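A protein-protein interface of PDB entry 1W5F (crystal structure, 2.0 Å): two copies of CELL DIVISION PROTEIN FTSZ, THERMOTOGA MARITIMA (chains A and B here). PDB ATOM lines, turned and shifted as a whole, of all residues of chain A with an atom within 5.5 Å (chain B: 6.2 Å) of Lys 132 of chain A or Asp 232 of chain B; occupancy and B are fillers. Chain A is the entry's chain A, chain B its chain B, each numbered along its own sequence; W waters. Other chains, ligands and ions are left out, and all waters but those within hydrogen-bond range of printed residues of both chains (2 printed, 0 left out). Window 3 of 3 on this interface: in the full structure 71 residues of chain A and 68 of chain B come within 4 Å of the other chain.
O of Met 230 of chain B lies within hydrogen-bond range of OG1 of Thr 170 of chain A, 2.8 Å away.
The backbone carbonyl oxygen of Met 230 of chain B lies close to the backbone carbonyl oxygen of Asp 169 of chain A (3.4 Å).
The side-chain amino group (NZ) of Lys 132 of chain A is in salt-bridge range of the side-chain carboxylate (OD1) of Asp 232 of chain B (2.7 Å).
OD1 of Asp 169 of chain A lies within hydrogen-bond range of N of Asp 232 of chain B.
The side-chain amino group of Lys 231 of chain B is in hydrogen-bond range of the backbone carbonyl oxygen of Ile 136 of chain A.
N of Ala 233 of chain B is in hydrogen-bond range of O of Asp 169 of chain A (2.8 Å).
The backbone NH of Gly 234 of chain B sits at hydrogen-bond distance from the backbone carbonyl oxygen of Asp 169 of chain A, at 2.8 Å.
OD2 of Asp 169 of chain A is in salt-bridge range of NZ of Lys 231 of chain B (2.9 Å).
The backbone carbonyl oxygen of Ile 136 of chain A lies within hydrogen-bond range of the side-chain hydroxyl of Thr 138 of chain A (2.8 Å).
The side-chain amino group (NZ) of Lys 132 of chain A is in salt-bridge range of the side-chain carboxylate (OD1) of Asp 169 of chain A (3.6 Å).
The backbone NH (N) of Lys 132 of chain A lies within hydrogen-bond range of the side-chain hydroxyl (OG1) of Thr 138 of chain A, at 3.4 Å.
The backbone carbonyl oxygen of Thr 138 of chain A is in hydrogen-bond range of the backbone NH of Thr 170 of chain A.
N of Thr 138 of chain A lies within hydrogen-bond range of OD2 of Asp 169 of chain A (2.8 Å).
O of Lys 231 of chain B lies within hydrogen-bond range of NH1 of Arg 327 of chain B (3.1 Å).
Thr 170 of chain A touches Ala 233 of chain B.
Thr 170 of chain A touches Gly 234 of chain B (CA to O, 3.4 Å).
Lys 132 of chain A touches just one residue of chain B: Asp 232.
Printed residues of chain A within 4 Å of Lys 231 of chain B: Ile 136 (3.4 Å) and Asp 169 (2.9 Å).
Of the printed residues of chain B, Ile 136 of chain A touches Lys 231 (3.4 Å).
Arg 327 of chain B touches none of the printed residues of chain A.
Ile 130 of chain A touches none of the printed residues of chain B.
Printed residues of chain B that touch a printed residue of chain A: Met 230, Lys 231, Asp 232, Ala 233 and Gly 234.
No position is printed for both chains.
Of the 10 pairs that touch across the chains among the printed residues, none has its exchanged pair printed and touching as well.
Water W2 lies within hydrogen-bond range of the backbone carbonyl oxygen (O) of Val 168 of chain A (2.7 Å), the backbone carbonyl oxygen (O) of Asp 169 of chain A (3.3 Å) and the backbone NH (N) of Gly 234 of chain B (3.3 Å).
Water W1 lies within hydrogen-bond range of the side-chain amino group of Lys 231 of chain B (2.8 Å) and the backbone carbonyl oxygen of Lys 132 of chain A (2.9 Å).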
ATOM      1  N   ILE A 127      32.353  -3.544  18.400  1.00  0.00           N
ATOM      2  CA  ILE A 127      33.156  -4.234  17.398  1.00  0.00           C
ATOM      3  C   ILE A 127      32.246  -4.900  16.361  1.00  0.00           C
ATOM      4  O   ILE A 127      32.547  -4.898  15.163  1.00  0.00           O
ATOM      5  CB  ILE A 127      34.059  -5.308  18.053  1.00  0.00           C
ATOM      6  CG1 ILE A 127      35.127  -4.626  18.916  1.00  0.00           C
ATOM      7  CG2 ILE A 127      34.709  -6.175  16.977  1.00  0.00           C
ATOM      8  CD1 ILE A 127      35.791  -5.540  19.923  1.00  0.00           C
ATOM      9  N   ALA A 128      31.133  -5.466  16.822  1.00  0.00           N
ATOM     10  CA  ALA A 128      30.192  -6.127  15.917  1.00  0.00           C
ATOM     11  C   ALA A 128      29.582  -5.098  14.973  1.00  0.00           C
ATOM     12  O   ALA A 128      29.440  -5.350  13.780  1.00  0.00           O
ATOM     13  CB  ALA A 128      29.094  -6.824  16.711  1.00  0.00           C
ATOM     14  N   LYS A 129      29.227  -3.938  15.519  1.00  0.00           N
ATOM     15  CA  LYS A 129      28.638  -2.857  14.730  1.00  0.00           C
ATOM     16  C   LYS A 129      29.579  -2.459  13.598  1.00  0.00           C
ATOM     17  O   LYS A 129      29.167  -2.350  12.440  1.00  0.00           O
ATOM     18  CB  LYS A 129      28.358  -1.639  15.622  1.00  0.00           C
ATOM     19  CG  LYS A 129      27.665  -0.484  14.898  1.00  0.00           C
ATOM     20  CD  LYS A 129      27.590   0.771  15.769  1.00  0.00           C
ATOM     21  CE  LYS A 129      28.978   1.376  15.984  1.00  0.00           C
ATOM     22  NZ  LYS A 129      28.955   2.625  16.797  1.00  0.00           N
ATOM     23  N   ILE A 130      30.846  -2.246  13.937  1.00  0.00           N
ATOM     24  CA  ILE A 130      31.857  -1.856  12.955  1.00  0.00           C
ATOM     25  C   ILE A 130      32.054  -2.920  11.871  1.00  0.00           C
ATOM     26  O   ILE A 130      32.100  -2.610  10.674  1.00  0.00           O
ATOM     27  CB  ILE A 130      33.208  -1.589  13.656  1.00  0.00           C
ATOM     28  CG1 ILE A 130      33.065  -0.398  14.608  1.00  0.00           C
ATOM     29  CG2 ILE A 130      34.294  -1.332  12.625  1.00  0.00           C
ATOM     30  CD1 ILE A 130      34.230  -0.235  15.567  1.00  0.00           C
ATOM     31  N   ALA A 131      32.168  -4.176  12.289  1.00  0.00           N
ATOM     32  CA  ALA A 131      32.364  -5.270  11.347  1.00  0.00           C
ATOM     33  C   ALA A 131      31.190  -5.410  10.380  1.00  0.00           C
ATOM     34  O   ALA A 131      31.381  -5.570   9.173  1.00  0.00           O
ATOM     35  CB  ALA A 131      32.574  -6.582  12.108  1.00  0.00           C
ATOM     36  N   LYS A 132      29.974  -5.350  10.908  1.00  0.00           N
ATOM     37  CA  LYS A 132      28.800  -5.496  10.063  1.00  0.00           C
ATOM     38  C   LYS A 132      28.690  -4.343   9.073  1.00  0.00           C
ATOM     39  O   LYS A 132      28.377  -4.557   7.900  1.00  0.00           O
ATOM     40  CB  LYS A 132      27.528  -5.588  10.912  1.00  0.00           C
ATOM     41  CG  LYS A 132      26.363  -6.250  10.183  1.00  0.00           C
ATOM     42  CD  LYS A 132      25.119  -6.310  11.059  1.00  0.00           C
ATOM     43  CE  LYS A 132      24.049  -7.205  10.444  1.00  0.00           C
ATOM     44  NZ  LYS A 132      23.713  -6.809   9.052  1.00  0.00           N
ATOM     45  N   GLU A 133      28.943  -3.121   9.537  1.00  0.00           N
ATOM     46  CA  GLU A 133      28.884  -1.964   8.650  1.00  0.00           C
ATOM     47  C   GLU A 133      29.878  -2.148   7.508  1.00  0.00           C
ATOM     48  O   GLU A 133      29.642  -1.682   6.394  1.00  0.00           O
ATOM     49  CB  GLU A 133      29.214  -0.673   9.407  1.00  0.00           C
ATOM     50  CG  GLU A 133      28.106  -0.186  10.337  1.00  0.00           C
ATOM     51  CD  GLU A 133      28.432   1.146  11.000  1.00  0.00           C
ATOM     52  OE1 GLU A 133      27.553   1.692  11.703  1.00  0.00           O
ATOM     53  OE2 GLU A 133      29.566   1.644  10.819  1.00  0.00           O
ATOM     54  N   MET A 134      30.983  -2.838   7.791  1.00  0.00           N
ATOM     55  CA  MET A 134      32.027  -3.085   6.797  1.00  0.00           C
ATOM     56  C   MET A 134      31.705  -4.215   5.818  1.00  0.00           C
ATOM     57  O   MET A 134      32.492  -4.507   4.920  1.00  0.00           O
ATOM     58  CB  MET A 134      33.361  -3.374   7.500  1.00  0.00           C
ATOM     59  CG  MET A 134      34.017  -2.142   8.119  1.00  0.00           C
ATOM     60  SD  MET A 134      35.522  -2.492   9.069  1.00  0.00           S
ATOM     61  CE  MET A 134      36.659  -2.959   7.761  1.00  0.00           C
ATOM     62  N   GLY A 135      30.553  -4.854   5.997  1.00  0.00           N
ATOM     63  CA  GLY A 135      30.163  -5.933   5.105  1.00  0.00           C
ATOM     64  C   GLY A 135      30.719  -7.298   5.474  1.00  0.00           C
ATOM     65  O   GLY A 135      30.632  -8.242   4.693  1.00  0.00           O
ATOM     66  N   ILE A 136      31.281  -7.410   6.671  1.00  0.00           N
ATOM     67  CA  ILE A 136      31.851  -8.670   7.141  1.00  0.00           C
ATOM     68  C   ILE A 136      30.771  -9.579   7.741  1.00  0.00           C
ATOM     69  O   ILE A 136      29.890  -9.103   8.451  1.00  0.00           O
ATOM     70  CB  ILE A 136      32.919  -8.399   8.227  1.00  0.00           C
ATOM     71  CG1 ILE A 136      34.005  -7.477   7.666  1.00  0.00           C
ATOM     72  CG2 ILE A 136      33.518  -9.714   8.724  1.00  0.00           C
ATOM     73  CD1 ILE A 136      35.048  -7.068   8.689  1.00  0.00           C
ATOM     74  N   THR A 138      29.308 -11.245  10.329  1.00  0.00           N
ATOM     75  CA  THR A 138      29.552 -11.073  11.757  1.00  0.00           C
ATOM     76  C   THR A 138      28.834 -12.050  12.689  1.00  0.00           C
ATOM     77  O   THR A 138      27.629 -11.939  12.928  1.00  0.00           O
ATOM     78  CB  THR A 138      29.202  -9.618  12.132  1.00  0.00           C
ATOM     79  OG1 THR A 138      29.866  -8.736  11.214  1.00  0.00           O
ATOM     80  CG2 THR A 138      29.635  -9.287  13.557  1.00  0.00           C
ATOM     81  N   HIS A 167      23.178  -5.099  16.084  1.00  0.00           N
ATOM     82  CA  HIS A 167      24.127  -5.101  14.974  1.00  0.00           C
ATOM     83  C   HIS A 167      25.025  -6.334  14.848  1.00  0.00           C
ATOM     84  O   HIS A 167      26.218  -6.263  15.118  1.00  0.00           O
ATOM     85  CB  HIS A 167      25.009  -3.850  15.050  1.00  0.00           C
ATOM     86  CG  HIS A 167      24.234  -2.572  15.109  1.00  0.00           C
ATOM     87  ND1 HIS A 167      23.395  -2.163  14.094  1.00  0.00           N
ATOM     88  CD2 HIS A 167      24.144  -1.628  16.076  1.00  0.00           C
ATOM     89  CE1 HIS A 167      22.820  -1.023  14.434  1.00  0.00           C
ATOM     90  NE2 HIS A 167      23.257  -0.677  15.631  1.00  0.00           N
ATOM     91  N   VAL A 168      24.445  -7.451  14.422  1.00  0.00           N
ATOM     92  CA  VAL A 168      25.186  -8.696  14.216  1.00  0.00           C
ATOM     93  C   VAL A 168      24.443  -9.510  13.173  1.00  0.00           C
ATOM     94  O   VAL A 168      23.262  -9.261  12.918  1.00  0.00           O
ATOM     95  CB  VAL A 168      25.272  -9.561  15.497  1.00  0.00           C
ATOM     96  CG1 VAL A 168      26.242  -8.947  16.483  1.00  0.00           C
ATOM     97  CG2 VAL A 168      23.886  -9.711  16.115  1.00  0.00           C
ATOM     98  N   ASP A 169      25.124 -10.474  12.560  1.00  0.00           N
ATOM     99  CA  ASP A 169      24.463 -11.315  11.570  1.00  0.00           C
ATOM    100  C   ASP A 169      23.828 -12.492  12.295  1.00  0.00           C
ATOM    101  O   ASP A 169      22.622 -12.716  12.193  1.00  0.00           O
ATOM    102  CB  ASP A 169      25.455 -11.796  10.504  1.00  0.00           C
ATOM    103  CG  ASP A 169      25.687 -10.755   9.426  1.00  0.00           C
ATOM    104  OD1 ASP A 169      24.690 -10.307   8.824  1.00  0.00           O
ATOM    105  OD2 ASP A 169      26.855 -10.384   9.175  1.00  0.00           O
ATOM    106  N   THR A 170      24.645 -13.231  13.040  1.00  0.00           N
ATOM    107  CA  THR A 170      24.166 -14.370  13.806  1.00  0.00           C
ATOM    108  C   THR A 170      24.664 -14.236  15.240  1.00  0.00           C
ATOM    109  O   THR A 170      25.857 -14.027  15.479  1.00  0.00           O
ATOM    110  CB  THR A 170      24.666 -15.708  13.213  1.00  0.00           C
ATOM    111  OG1 THR A 170      24.016 -15.947  11.959  1.00  0.00           O
ATOM    112  CG2 THR A 170      24.351 -16.858  14.151  1.00  0.00           C
ATOM    113  N   GLU B 227      27.162 -18.317   4.372  1.00  0.00           N
ATOM    114  CA  GLU B 227      26.790 -16.908   4.381  1.00  0.00           C
ATOM    115  C   GLU B 227      25.285 -16.722   4.170  1.00  0.00           C
ATOM    116  O   GLU B 227      24.633 -15.986   4.912  1.00  0.00           O
ATOM    117  CB  GLU B 227      27.554 -16.147   3.294  1.00  0.00           C
ATOM    118  CG  GLU B 227      27.351 -14.639   3.354  1.00  0.00           C
ATOM    119  CD  GLU B 227      28.008 -13.898   2.202  1.00  0.00           C
ATOM    120  OE1 GLU B 227      28.067 -12.651   2.262  1.00  0.00           O
ATOM    121  OE2 GLU B 227      28.456 -14.554   1.237  1.00  0.00           O
ATOM    122  N   VAL B 229      22.877 -18.473   4.943  1.00  0.00           N
ATOM    123  CA  VAL B 229      22.094 -18.834   6.119  1.00  0.00           C
ATOM    124  C   VAL B 229      22.407 -18.021   7.378  1.00  0.00           C
ATOM    125  O   VAL B 229      21.546 -17.850   8.242  1.00  0.00           O
ATOM    126  CB  VAL B 229      22.272 -20.323   6.466  1.00  0.00           C
ATOM    127  CG1 VAL B 229      21.424 -20.669   7.674  1.00  0.00           C
ATOM    128  CG2 VAL B 229      21.889 -21.188   5.272  1.00  0.00           C
ATOM    129  N   MET B 230      23.629 -17.515   7.489  1.00  0.00           N
ATOM    130  CA  MET B 230      24.003 -16.757   8.678  1.00  0.00           C
ATOM    131  C   MET B 230      23.861 -15.243   8.571  1.00  0.00           C
ATOM    132  O   MET B 230      23.887 -14.545   9.585  1.00  0.00           O
ATOM    133  CB  MET B 230      25.433 -17.117   9.092  1.00  0.00           C
ATOM    134  CG  MET B 230      25.594 -18.582   9.477  1.00  0.00           C
ATOM    135  SD  MET B 230      27.206 -18.988  10.171  1.00  0.00           S
ATOM    136  CE  MET B 230      26.902 -18.673  11.900  1.00  0.00           C
ATOM    137  N   LYS B 231      23.700 -14.729   7.357  1.00  0.00           N
ATOM    138  CA  LYS B 231      23.572 -13.285   7.172  1.00  0.00           C
ATOM    139  C   LYS B 231      22.236 -12.772   7.711  1.00  0.00           C
ATOM    140  O   LYS B 231      21.179 -13.283   7.351  1.00  0.00           O
ATOM    141  CB  LYS B 231      23.705 -12.933   5.690  1.00  0.00           C
ATOM    142  CG  LYS B 231      24.099 -11.490   5.432  1.00  0.00           C
ATOM    143  CD  LYS B 231      25.482 -11.199   6.001  1.00  0.00           C
ATOM    144  CE  LYS B 231      25.886  -9.747   5.797  1.00  0.00           C
ATOM    145  NZ  LYS B 231      27.183  -9.432   6.467  1.00  0.00           N
ATOM    146  N   ASP B 232      22.292 -11.762   8.577  1.00  0.00           N
ATOM    147  CA  ASP B 232      21.088 -11.184   9.170  1.00  0.00           C
ATOM    148  C   ASP B 232      20.140 -12.260   9.698  1.00  0.00           C
ATOM    149  O   ASP B 232      18.918 -12.118   9.620  1.00  0.00           O
ATOM    150  CB  ASP B 232      20.351 -10.320   8.139  1.00  0.00           C
ATOM    151  CG  ASP B 232      21.180  -9.141   7.665  1.00  0.00           C
ATOM    152  OD1 ASP B 232      21.606  -8.331   8.513  1.00  0.00           O
ATOM    153  OD2 ASP B 232      21.402  -9.021   6.445  1.00  0.00           O
ATOM    154  N   ALA B 233      20.708 -13.329  10.248  1.00  0.00           N
ATOM    155  CA  ALA B 233      19.914 -14.436  10.773  1.00  0.00           C
ATOM    156  C   ALA B 233      19.333 -14.168  12.160  1.00  0.00           C
ATOM    157  O   ALA B 233      18.282 -14.705  12.504  1.00  0.00           O
ATOM    158  CB  ALA B 233      20.757 -15.709  10.799  1.00  0.00           C
ATOM    159  N   GLY B 234      20.011 -13.344  12.954  1.00  0.00           N
ATOM    160  CA  GLY B 234      19.525 -13.051  14.292  1.00  0.00           C
ATOM    161  C   GLY B 234      19.985 -14.073  15.322  1.00  0.00           C
ATOM    162  O   GLY B 234      21.066 -14.650  15.186  1.00  0.00           O
ATOM    163  N   ARG B 327      16.426 -17.888  12.698  1.00  0.00           N
ATOM    164  CA  ARG B 327      15.185 -17.281  12.239  1.00  0.00           C
ATOM    165  C   ARG B 327      13.950 -17.802  12.955  1.00  0.00           C
ATOM    166  O   ARG B 327      13.131 -18.515  12.378  1.00  0.00           O
ATOM    167  CB  ARG B 327      15.051 -17.471  10.729  1.00  0.00           C
ATOM    168  CG  ARG B 327      16.193 -16.827   9.966  1.00  0.00           C
ATOM    169  CD  ARG B 327      15.979 -16.859   8.471  1.00  0.00           C
ATOM    170  NE  ARG B 327      17.000 -16.080   7.777  1.00  0.00           N
ATOM    171  CZ  ARG B 327      18.298 -16.365   7.789  1.00  0.00           C
ATOM    172  NH1 ARG B 327      19.155 -15.596   7.130  1.00  0.00           N
ATOM    173  NH2 ARG B 327      18.739 -17.426   8.456  1.00  0.00           N
HETATM  174  O   HOH W   1      26.753  -6.637   6.588  1.00  0.00           O
HETATM  175  O   HOH W   2      20.753 -10.130  12.978  1.00  0.00           O
